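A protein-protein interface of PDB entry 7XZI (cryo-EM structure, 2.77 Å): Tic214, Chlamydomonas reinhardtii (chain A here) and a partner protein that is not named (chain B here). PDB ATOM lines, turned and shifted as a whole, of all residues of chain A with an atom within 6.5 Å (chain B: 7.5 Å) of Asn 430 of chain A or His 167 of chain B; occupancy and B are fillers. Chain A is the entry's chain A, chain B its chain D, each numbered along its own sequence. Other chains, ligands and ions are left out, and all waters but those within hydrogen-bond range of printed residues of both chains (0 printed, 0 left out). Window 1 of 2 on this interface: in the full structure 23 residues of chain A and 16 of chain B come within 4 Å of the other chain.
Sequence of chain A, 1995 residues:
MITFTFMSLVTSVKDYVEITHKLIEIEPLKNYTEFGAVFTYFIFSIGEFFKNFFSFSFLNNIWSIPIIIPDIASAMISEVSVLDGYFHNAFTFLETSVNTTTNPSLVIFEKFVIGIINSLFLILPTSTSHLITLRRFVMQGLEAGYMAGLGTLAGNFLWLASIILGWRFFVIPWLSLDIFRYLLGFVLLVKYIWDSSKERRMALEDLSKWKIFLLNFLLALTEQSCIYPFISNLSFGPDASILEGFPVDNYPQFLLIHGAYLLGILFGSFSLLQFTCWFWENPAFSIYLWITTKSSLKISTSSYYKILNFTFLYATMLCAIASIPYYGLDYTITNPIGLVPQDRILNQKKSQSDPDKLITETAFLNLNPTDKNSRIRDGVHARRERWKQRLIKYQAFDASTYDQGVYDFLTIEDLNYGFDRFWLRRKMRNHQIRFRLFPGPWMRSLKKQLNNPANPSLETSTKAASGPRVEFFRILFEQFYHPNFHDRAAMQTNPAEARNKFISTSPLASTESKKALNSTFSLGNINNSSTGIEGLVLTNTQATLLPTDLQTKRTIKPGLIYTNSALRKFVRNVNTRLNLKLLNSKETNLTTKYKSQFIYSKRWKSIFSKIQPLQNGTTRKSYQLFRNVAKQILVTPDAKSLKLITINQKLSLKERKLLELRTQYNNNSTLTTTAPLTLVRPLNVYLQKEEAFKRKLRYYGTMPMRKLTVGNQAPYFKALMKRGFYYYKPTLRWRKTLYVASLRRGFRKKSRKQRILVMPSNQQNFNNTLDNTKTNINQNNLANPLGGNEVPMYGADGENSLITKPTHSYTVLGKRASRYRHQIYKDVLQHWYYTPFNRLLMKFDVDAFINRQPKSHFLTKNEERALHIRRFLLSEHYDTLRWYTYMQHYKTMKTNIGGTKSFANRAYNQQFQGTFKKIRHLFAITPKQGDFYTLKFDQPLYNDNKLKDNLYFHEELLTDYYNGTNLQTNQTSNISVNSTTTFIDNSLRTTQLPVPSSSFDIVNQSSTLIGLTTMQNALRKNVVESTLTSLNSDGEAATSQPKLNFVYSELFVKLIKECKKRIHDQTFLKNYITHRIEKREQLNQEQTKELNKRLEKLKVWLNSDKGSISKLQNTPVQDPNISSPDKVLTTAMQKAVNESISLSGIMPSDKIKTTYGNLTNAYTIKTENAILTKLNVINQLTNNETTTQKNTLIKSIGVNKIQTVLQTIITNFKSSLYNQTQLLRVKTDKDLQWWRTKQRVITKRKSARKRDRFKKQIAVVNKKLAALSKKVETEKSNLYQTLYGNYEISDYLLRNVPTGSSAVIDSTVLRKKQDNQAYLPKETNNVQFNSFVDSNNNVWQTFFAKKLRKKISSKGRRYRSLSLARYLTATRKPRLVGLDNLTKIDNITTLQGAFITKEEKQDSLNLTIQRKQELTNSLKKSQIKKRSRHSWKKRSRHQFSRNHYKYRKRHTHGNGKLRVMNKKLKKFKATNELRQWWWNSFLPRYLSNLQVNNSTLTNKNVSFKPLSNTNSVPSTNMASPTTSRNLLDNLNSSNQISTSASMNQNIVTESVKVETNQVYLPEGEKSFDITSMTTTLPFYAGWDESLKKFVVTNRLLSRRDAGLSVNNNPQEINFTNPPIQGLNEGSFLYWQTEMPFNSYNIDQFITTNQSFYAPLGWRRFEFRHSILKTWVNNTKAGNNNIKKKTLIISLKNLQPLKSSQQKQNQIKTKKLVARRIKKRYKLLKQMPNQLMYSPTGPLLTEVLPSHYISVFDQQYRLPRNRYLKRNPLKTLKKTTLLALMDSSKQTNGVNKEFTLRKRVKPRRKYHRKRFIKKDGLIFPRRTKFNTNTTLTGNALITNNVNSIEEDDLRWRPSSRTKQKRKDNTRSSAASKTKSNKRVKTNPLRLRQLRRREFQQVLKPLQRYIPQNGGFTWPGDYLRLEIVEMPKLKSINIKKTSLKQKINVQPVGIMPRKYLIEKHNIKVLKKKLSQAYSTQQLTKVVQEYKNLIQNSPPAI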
ATOM      1  N   ARG A 386       5.516  -8.924 -31.849  1.00  0.00           N
ATOM      2  CA  ARG A 386       6.564  -8.432 -30.965  1.00  0.00           C
ATOM      3  C   ARG A 386       6.027  -7.844 -29.667  1.00  0.00           C
ATOM      4  O   ARG A 386       6.804  -7.668 -28.724  1.00  0.00           O
ATOM      5  CB  ARG A 386       7.408  -7.376 -31.680  1.00  0.00           C
ATOM      6  CG  ARG A 386       8.222  -7.901 -32.842  1.00  0.00           C
ATOM      7  CD  ARG A 386       9.091  -6.801 -33.423  1.00  0.00           C
ATOM      8  NE  ARG A 386       8.293  -5.706 -33.954  1.00  0.00           N
ATOM      9  CZ  ARG A 386       8.793  -4.566 -34.417  1.00  0.00           C
ATOM     10  NH1 ARG A 386      10.095  -4.332 -34.413  1.00  0.00           N
ATOM     11  NH2 ARG A 386       7.967  -3.642 -34.893  1.00  0.00           N
ATOM     12  N   ARG A 390       7.475 -11.694 -24.704  1.00  0.00           N
ATOM     13  CA  ARG A 390       7.758 -12.337 -23.426  1.00  0.00           C
ATOM     14  C   ARG A 390       6.647 -13.295 -23.018  1.00  0.00           C
ATOM     15  O   ARG A 390       6.902 -14.264 -22.294  1.00  0.00           O
ATOM     16  CB  ARG A 390       7.974 -11.276 -22.347  1.00  0.00           C
ATOM     17  CG  ARG A 390       9.176 -10.384 -22.600  1.00  0.00           C
ATOM     18  CD  ARG A 390      10.454 -11.205 -22.668  1.00  0.00           C
ATOM     19  NE  ARG A 390      11.190 -10.977 -23.905  1.00  0.00           N
ATOM     20  CZ  ARG A 390      12.271 -11.659 -24.270  1.00  0.00           C
ATOM     21  NH1 ARG A 390      12.769 -12.621 -23.512  1.00  0.00           N
ATOM     22  NH2 ARG A 390      12.861 -11.368 -25.424  1.00  0.00           N
ATOM     23  N   TRP A 423       5.616  -1.428 -20.180  1.00  0.00           N
ATOM     24  CA  TRP A 423       6.894  -2.122 -20.046  1.00  0.00           C
ATOM     25  C   TRP A 423       6.801  -3.570 -20.504  1.00  0.00           C
ATOM     26  O   TRP A 423       7.797  -4.141 -20.962  1.00  0.00           O
ATOM     27  CB  TRP A 423       7.380  -2.058 -18.601  1.00  0.00           C
ATOM     28  CG  TRP A 423       8.607  -2.864 -18.351  1.00  0.00           C
ATOM     29  CD1 TRP A 423       8.671  -4.110 -17.802  1.00  0.00           C
ATOM     30  CD2 TRP A 423       9.955  -2.486 -18.647  1.00  0.00           C
ATOM     31  NE1 TRP A 423       9.976  -4.531 -17.735  1.00  0.00           N
ATOM     32  CE2 TRP A 423      10.784  -3.550 -18.247  1.00  0.00           C
ATOM     33  CE3 TRP A 423      10.539  -1.348 -19.209  1.00  0.00           C
ATOM     34  CZ2 TRP A 423      12.168  -3.511 -18.391  1.00  0.00           C
ATOM     35  CZ3 TRP A 423      11.913  -1.311 -19.351  1.00  0.00           C
ATOM     36  CH2 TRP A 423      12.713  -2.386 -18.944  1.00  0.00           C
ATOM     37  N   ARG A 426       7.954  -4.103 -24.364  1.00  0.00           N
ATOM     38  CA  ARG A 426       9.137  -3.320 -24.695  1.00  0.00           C
ATOM     39  C   ARG A 426       9.853  -3.805 -25.950  1.00  0.00           C
ATOM     40  O   ARG A 426      10.764  -3.116 -26.422  1.00  0.00           O
ATOM     41  CB  ARG A 426      10.109  -3.330 -23.516  1.00  0.00           C
ATOM     42  CG  ARG A 426      10.560  -4.721 -23.110  1.00  0.00           C
ATOM     43  CD  ARG A 426      11.317  -4.696 -21.795  1.00  0.00           C
ATOM     44  NE  ARG A 426      11.770  -6.023 -21.403  1.00  0.00           N
ATOM     45  CZ  ARG A 426      11.038  -6.895 -20.720  1.00  0.00           C
ATOM     46  NH1 ARG A 426       9.804  -6.612 -20.337  1.00  0.00           N
ATOM     47  NH2 ARG A 426      11.556  -8.081 -20.417  1.00  0.00           N
ATOM     48  N   LYS A 427       9.478  -4.961 -26.496  1.00  0.00           N
ATOM     49  CA  LYS A 427      10.160  -5.475 -27.677  1.00  0.00           C
ATOM     50  C   LYS A 427       9.726  -4.779 -28.959  1.00  0.00           C
ATOM     51  O   LYS A 427      10.406  -4.915 -29.981  1.00  0.00           O
ATOM     52  CB  LYS A 427       9.931  -6.983 -27.803  1.00  0.00           C
ATOM     53  CG  LYS A 427      10.349  -7.777 -26.572  1.00  0.00           C
ATOM     54  CD  LYS A 427      11.806  -7.528 -26.208  1.00  0.00           C
ATOM     55  CE  LYS A 427      12.748  -8.039 -27.287  1.00  0.00           C
ATOM     56  NZ  LYS A 427      14.176  -7.812 -26.932  1.00  0.00           N
ATOM     57  N   MET A 428       8.613  -4.040 -28.930  1.00  0.00           N
ATOM     58  CA  MET A 428       8.159  -3.317 -30.113  1.00  0.00           C
ATOM     59  C   MET A 428       9.085  -2.167 -30.482  1.00  0.00           C
ATOM     60  O   MET A 428       9.041  -1.691 -31.621  1.00  0.00           O
ATOM     61  CB  MET A 428       6.742  -2.785 -29.890  1.00  0.00           C
ATOM     62  CG  MET A 428       5.671  -3.857 -29.812  1.00  0.00           C
ATOM     63  SD  MET A 428       5.241  -4.537 -31.426  1.00  0.00           S
ATOM     64  CE  MET A 428       4.592  -3.084 -32.245  1.00  0.00           C
ATOM     65  N   ARG A 429       9.915  -1.709 -29.549  1.00  0.00           N
ATOM     66  CA  ARG A 429      10.789  -0.559 -29.749  1.00  0.00           C
ATOM     67  C   ARG A 429      12.263  -0.946 -29.663  1.00  0.00           C
ATOM     68  O   ARG A 429      13.070  -0.248 -29.048  1.00  0.00           O
ATOM     69  CB  ARG A 429      10.459   0.537 -28.741  1.00  0.00           C
ATOM     70  CG  ARG A 429       9.967   0.008 -27.403  1.00  0.00           C
ATOM     71  CD  ARG A 429       9.327   1.104 -26.571  1.00  0.00           C
ATOM     72  NE  ARG A 429       8.580   0.563 -25.444  1.00  0.00           N
ATOM     73  CZ  ARG A 429       7.303   0.199 -25.498  1.00  0.00           C
ATOM     74  NH1 ARG A 429       6.601   0.304 -26.614  1.00  0.00           N
ATOM     75  NH2 ARG A 429       6.720  -0.283 -24.404  1.00  0.00           N
ATOM     76  N   ASN A 430      12.626  -2.068 -30.278  1.00  0.00           N
ATOM     77  CA  ASN A 430      14.003  -2.541 -30.323  1.00  0.00           C
ATOM     78  C   ASN A 430      14.506  -2.436 -31.756  1.00  0.00           C
ATOM     79  O   ASN A 430      13.895  -2.993 -32.674  1.00  0.00           O
ATOM     80  CB  ASN A 430      14.106  -3.980 -29.817  1.00  0.00           C
ATOM     81  CG  ASN A 430      15.531  -4.386 -29.487  1.00  0.00           C
ATOM     82  OD1 ASN A 430      16.490  -3.830 -30.023  1.00  0.00           O
ATOM     83  ND2 ASN A 430      15.677  -5.362 -28.599  1.00  0.00           N
ATOM     84  N   HIS A 431      15.616  -1.726 -31.944  1.00  0.00           N
ATOM     85  CA  HIS A 431      16.176  -1.526 -33.273  1.00  0.00           C
ATOM     86  C   HIS A 431      16.772  -2.826 -33.796  1.00  0.00           C
ATOM     87  O   HIS A 431      17.408  -3.574 -33.048  1.00  0.00           O
ATOM     88  CB  HIS A 431      17.240  -0.430 -33.246  1.00  0.00           C
ATOM     89  CG  HIS A 431      17.813  -0.114 -34.593  1.00  0.00           C
ATOM     90  ND1 HIS A 431      17.114   0.586 -35.553  1.00  0.00           N
ATOM     91  CD2 HIS A 431      19.016  -0.405 -35.142  1.00  0.00           C
ATOM     92  CE1 HIS A 431      17.862   0.714 -36.634  1.00  0.00           C
ATOM     93  NE2 HIS A 431      19.021   0.120 -36.411  1.00  0.00           N
ATOM     94  N   GLN A 432      16.563  -3.093 -35.083  1.00  0.00           N
ATOM     95  CA  GLN A 432      17.053  -4.300 -35.728  1.00  0.00           C
ATOM     96  C   GLN A 432      17.881  -3.937 -36.954  1.00  0.00           C
ATOM     97  O   GLN A 432      17.704  -2.871 -37.551  1.00  0.00           O
ATOM     98  CB  GLN A 432      15.897  -5.222 -36.130  1.00  0.00           C
ATOM     99  CG  GLN A 432      15.080  -5.737 -34.957  1.00  0.00           C
ATOM    100  CD  GLN A 432      13.844  -6.495 -35.396  1.00  0.00           C
ATOM    101  OE1 GLN A 432      13.182  -6.119 -36.363  1.00  0.00           O
ATOM    102  NE2 GLN A 432      13.529  -7.573 -34.688  1.00  0.00           N
ATOM    103  N   ARG A 434      18.909  -4.711 -40.772  1.00  0.00           N
ATOM    104  CA  ARG A 434      18.328  -5.318 -41.961  1.00  0.00           C
ATOM    105  C   ARG A 434      18.939  -4.685 -43.201  1.00  0.00           C
ATOM    106  O   ARG A 434      19.200  -3.480 -43.229  1.00  0.00           O
ATOM    107  CB  ARG A 434      16.803  -5.162 -41.977  1.00  0.00           C
ATOM    108  CG  ARG A 434      16.326  -3.721 -41.877  1.00  0.00           C
ATOM    109  CD  ARG A 434      14.811  -3.638 -41.821  1.00  0.00           C
ATOM    110  NE  ARG A 434      14.274  -4.298 -40.640  1.00  0.00           N
ATOM    111  CZ  ARG A 434      14.131  -3.716 -39.454  1.00  0.00           C
ATOM    112  NH1 ARG A 434      14.486  -2.457 -39.255  1.00  0.00           N
ATOM    113  NH2 ARG A 434      13.619  -4.414 -38.446  1.00  0.00           N
ATOM    114  N   HIS A 822      19.502  -3.318 -15.982  1.00  0.00           N
ATOM    115  CA  HIS A 822      18.120  -3.477 -16.419  1.00  0.00           C
ATOM    116  C   HIS A 822      17.145  -2.907 -15.397  1.00  0.00           C
ATOM    117  O   HIS A 822      16.199  -2.199 -15.768  1.00  0.00           O
ATOM    118  CB  HIS A 822      17.834  -4.958 -16.678  1.00  0.00           C
ATOM    119  CG  HIS A 822      16.581  -5.209 -17.459  1.00  0.00           C
ATOM    120  ND1 HIS A 822      16.539  -5.159 -18.837  1.00  0.00           N
ATOM    121  CD2 HIS A 822      15.329  -5.526 -17.056  1.00  0.00           C
ATOM    122  CE1 HIS A 822      15.313  -5.429 -19.247  1.00  0.00           C
ATOM    123  NE2 HIS A 822      14.560  -5.654 -18.186  1.00  0.00           N
ATOM    124  N   TYR A 825      17.405   0.938 -15.463  1.00  0.00           N
ATOM    125  CA  TYR A 825      16.742   1.468 -16.650  1.00  0.00           C
ATOM    126  C   TYR A 825      15.228   1.429 -16.490  1.00  0.00           C
ATOM    127  O   TYR A 825      14.530   2.389 -16.840  1.00  0.00           O
ATOM    128  CB  TYR A 825      17.184   0.676 -17.882  1.00  0.00           C
ATOM    129  CG  TYR A 825      16.698   1.218 -19.210  1.00  0.00           C
ATOM    130  CD1 TYR A 825      17.408   2.205 -19.881  1.00  0.00           C
ATOM    131  CD2 TYR A 825      15.545   0.726 -19.803  1.00  0.00           C
ATOM    132  CE1 TYR A 825      16.974   2.695 -21.098  1.00  0.00           C
ATOM    133  CE2 TYR A 825      15.106   1.207 -21.021  1.00  0.00           C
ATOM    134  CZ  TYR A 825      15.823   2.194 -21.663  1.00  0.00           C
ATOM    135  OH  TYR A 825      15.389   2.681 -22.874  1.00  0.00           O
ATOM    136  N   THR B 164      22.322   1.167 -30.125  1.00  0.00           N
ATOM    137  CA  THR B 164      21.333   2.223 -30.310  1.00  0.00           C
ATOM    138  C   THR B 164      20.517   2.500 -29.052  1.00  0.00           C
ATOM    139  O   THR B 164      19.573   3.294 -29.105  1.00  0.00           O
ATOM    140  CB  THR B 164      20.393   1.873 -31.467  1.00  0.00           C
ATOM    141  OG1 THR B 164      19.826   0.575 -31.251  1.00  0.00           O
ATOM    142  CG2 THR B 164      21.148   1.876 -32.783  1.00  0.00           C
ATOM    143  N   LEU B 165      20.857   1.858 -27.937  1.00  0.00           N
ATOM    144  CA  LEU B 165      20.135   1.974 -26.660  1.00  0.00           C
ATOM    145  C   LEU B 165      18.700   1.511 -26.908  1.00  0.00           C
ATOM    146  O   LEU B 165      18.507   0.447 -27.517  1.00  0.00           O
ATOM    147  CB  LEU B 165      20.291   3.380 -26.091  1.00  0.00           C
ATOM    148  CG  LEU B 165      20.100   3.486 -24.574  1.00  0.00           C
ATOM    149  CD1 LEU B 165      21.307   4.138 -23.922  1.00  0.00           C
ATOM    150  CD2 LEU B 165      18.824   4.238 -24.216  1.00  0.00           C
ATOM    151  N   GLY B 166      17.683   2.257 -26.487  1.00  0.00           N
ATOM    152  CA  GLY B 166      16.337   1.726 -26.500  1.00  0.00           C
ATOM    153  C   GLY B 166      16.263   0.520 -25.588  1.00  0.00           C
ATOM    154  O   GLY B 166      16.319   0.653 -24.361  1.00  0.00           O
ATOM    155  N   HIS B 167      16.138  -0.665 -26.182  1.00  0.00           N
ATOM    156  CA  HIS B 167      16.309  -1.923 -25.473  1.00  0.00           C
ATOM    157  C   HIS B 167      17.593  -2.642 -25.865  1.00  0.00           C
ATOM    158  O   HIS B 167      17.895  -3.698 -25.297  1.00  0.00           O
ATOM    159  CB  HIS B 167      15.108  -2.844 -25.733  1.00  0.00           C
ATOM    160  CG  HIS B 167      14.947  -3.934 -24.719  1.00  0.00           C
ATOM    161  ND1 HIS B 167      14.810  -3.679 -23.371  1.00  0.00           N
ATOM    162  CD2 HIS B 167      14.895  -5.281 -24.855  1.00  0.00           C
ATOM    163  CE1 HIS B 167      14.684  -4.821 -22.721  1.00  0.00           C
ATOM    164  NE2 HIS B 167      14.732  -5.808 -23.597  1.00  0.00           N
ATOM    165  N   ALA B 168      18.349  -2.100 -26.822  1.00  0.00           N
ATOM    166  CA  ALA B 168      19.544  -2.785 -27.307  1.00  0.00           C
ATOM    167  C   ALA B 168      20.666  -2.753 -26.275  1.00  0.00           C
ATOM    168  O   ALA B 168      21.284  -3.783 -25.983  1.00  0.00           O
ATOM    169  CB  ALA B 168      20.005  -2.165 -28.625  1.00  0.00           C
ATOM    170  N   LYS B 169      20.943  -1.577 -25.708  1.00  0.00           N
ATOM    171  CA  LYS B 169      22.067  -1.439 -24.790  1.00  0.00           C
ATOM    172  C   LYS B 169      21.863  -2.195 -23.485  1.00  0.00           C
ATOM    173  O   LYS B 169      22.838  -2.437 -22.767  1.00  0.00           O
ATOM    174  CB  LYS B 169      22.345   0.035 -24.493  1.00  0.00           C
ATOM    175  CG  LYS B 169      23.748   0.292 -23.961  1.00  0.00           C
ATOM    176  CD  LYS B 169      23.994   1.765 -23.696  1.00  0.00           C
ATOM    177  N   ASP B 170      20.627  -2.574 -23.158  1.00  0.00           N
ATOM    178  CA  ASP B 170      20.410  -3.443 -22.010  1.00  0.00           C
ATOM    179  C   ASP B 170      20.888  -4.864 -22.269  1.00  0.00           C
ATOM    180  O   ASP B 170      20.826  -5.697 -21.357  1.00  0.00           O
ATOM    181  CB  ASP B 170      18.935  -3.450 -21.616  1.00  0.00           C
ATOM    182  CG  ASP B 170      18.526  -2.193 -20.878  1.00  0.00           C
ATOM    183  OD1 ASP B 170      19.407  -1.352 -20.599  1.00  0.00           O
ATOM    184  OD2 ASP B 170      17.323  -2.046 -20.578  1.00  0.00           O
ATOM    185  N   THR B 171      21.358  -5.158 -23.484  1.00  0.00           N
ATOM    186  CA  THR B 171      21.848  -6.481 -23.852  1.00  0.00           C
ATOM    187  C   THR B 171      20.795  -7.555 -23.601  1.00  0.00           C
ATOM    188  O   THR B 171      21.099  -8.619 -23.058  1.00  0.00           O
ATOM    189  CB  THR B 171      23.149  -6.816 -23.113  1.00  0.00           C
ATOM    190  OG1 THR B 171      23.862  -5.605 -22.834  1.00  0.00           O
ATOM    191  CG2 THR B 171      24.031  -7.715 -23.962  1.00  0.00           C
ATOM    192  N   SER B 172      19.547  -7.258 -23.977  1.00  0.00           N
ATOM    193  CA  SER B 172      18.404  -8.124 -23.713  1.00  0.00           C
ATOM    194  C   SER B 172      18.337  -8.481 -22.235  1.00  0.00           C
ATOM    195  O   SER B 172      18.569  -7.628 -21.374  1.00  0.00           O
ATOM    196  CB  SER B 172      18.467  -9.388 -24.574  1.00  0.00           C
ATOM    197  N   MET B 173      18.026  -9.737 -21.930  1.00  0.00           N
ATOM    198  CA  MET B 173      17.957 -10.215 -20.556  1.00  0.00           C
ATOM    199  C   MET B 173      19.061 -11.237 -20.334  1.00  0.00           C
ATOM    200  O   MET B 173      19.130 -12.245 -21.047  1.00  0.00           O
ATOM    201  CB  MET B 173      16.587 -10.824 -20.247  1.00  0.00           C
ATOM    202  CG  MET B 173      15.523  -9.806 -19.865  1.00  0.00           C
ATOM    203  SD  MET B 173      15.138  -8.651 -21.191  1.00  0.00           S
ATOM    204  CE  MET B 173      14.738  -9.785 -22.519  1.00  0.00           C
ATOM    205  N   ASP B 179      22.412 -12.109 -27.726  1.00  0.00           N
ATOM    206  CA  ASP B 179      23.428 -11.197 -27.206  1.00  0.00           C
ATOM    207  C   ASP B 179      23.463 -11.235 -25.682  1.00  0.00           C
ATOM    208  O   ASP B 179      24.110 -12.097 -25.088  1.00  0.00           O
ATOM    209  CB  ASP B 179      23.176  -9.764 -27.688  1.00  0.00           C
ATOM    210  CG  ASP B 179      21.853  -9.207 -27.204  1.00  0.00           C
ATOM    211  OD1 ASP B 179      20.902  -9.996 -27.023  1.00  0.00           O
ATOM    212  OD2 ASP B 179      21.764  -7.977 -27.005  1.00  0.00           O
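O of Gly 166 of chain B sits at hydrogen-bond distance from OH of Tyr 825 of chain A (2.7 Å). The guanidinium group (NH2) of Arg 426 of chain A sits at hydrogen-bond distance from the side-chain sulfur (SD) of Met 173 of chain B (3.7 Å).
ND2 of Asn 430 of chain A lies close to NZ of Lys 427 of chain A, 3.3 Å away. The backbone carbonyl oxygen (O) of Trp 423 of chain A is in hydrogen-bond range of the guanidinium group (NH1) of Arg 426 of chain A. A ring nitrogen (NE2) of His 167 of chain B lies within hydrogen-bond range of the side-chain sulfur (SD) of Met 173 of chain B, 3.7 Å away.
Hydrophobic or aromatic side chains of chain A within 4 Å of the printed part of chain B: His 431, His 822 and Tyr 825. Along chain A the printed residues that touch a printed residue of chain B span positions 390 to 825.
Of the printed residues of chain B, Arg 426 of chain A touches His 167 and Met 173. Asn 430 of chain A touches just one residue of chain B: His 167. Of the printed residues of chain B, His 431 of chain A touches Thr 164. Of the printed residues of chain B, Tyr 825 of chain A touches Leu 165, Gly 166 and Asp 170. Of chain A, only Arg 426 (3.4 Å), Lys 427 (3.4 Å), Asn 430 (3.8 Å) and His 822 (3.6 Å) come within 4 Å of His 167 of chain B. The nearest residue of chain A that does not touch His 167 of chain B is Arg 429 of chain A (4.2 Å). The nearest printed residue of chain B that does not touch Arg 426 of chain A is Gly 166 of chain B (6.6 Å).
Arg 390 of chain A touches Met 173 of chain B. Arg 426 of chain A touches His 167 of chain B. Lys 427 of chain A touches His 167 of chain B. Asn 430 of chain A touches His 167 of chain B (ND2 to CD2, 3.8 Å). Thr 164 of chain B touches His 431 of chain A. His 167 of chain B touches His 822 of chain A (CE1 to CE1, 3.6 Å). His 822 of chain A touches Asp 170 of chain B. CE1 of His 822 of chain A touches SD of Met 173 of chain B, 3.8 Å away. Leu 165 of chain B touches Tyr 825 of chain A (CD2 to CE1, 3.9 Å). Tyr 825 of chain A touches Asp 170 of chain B.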
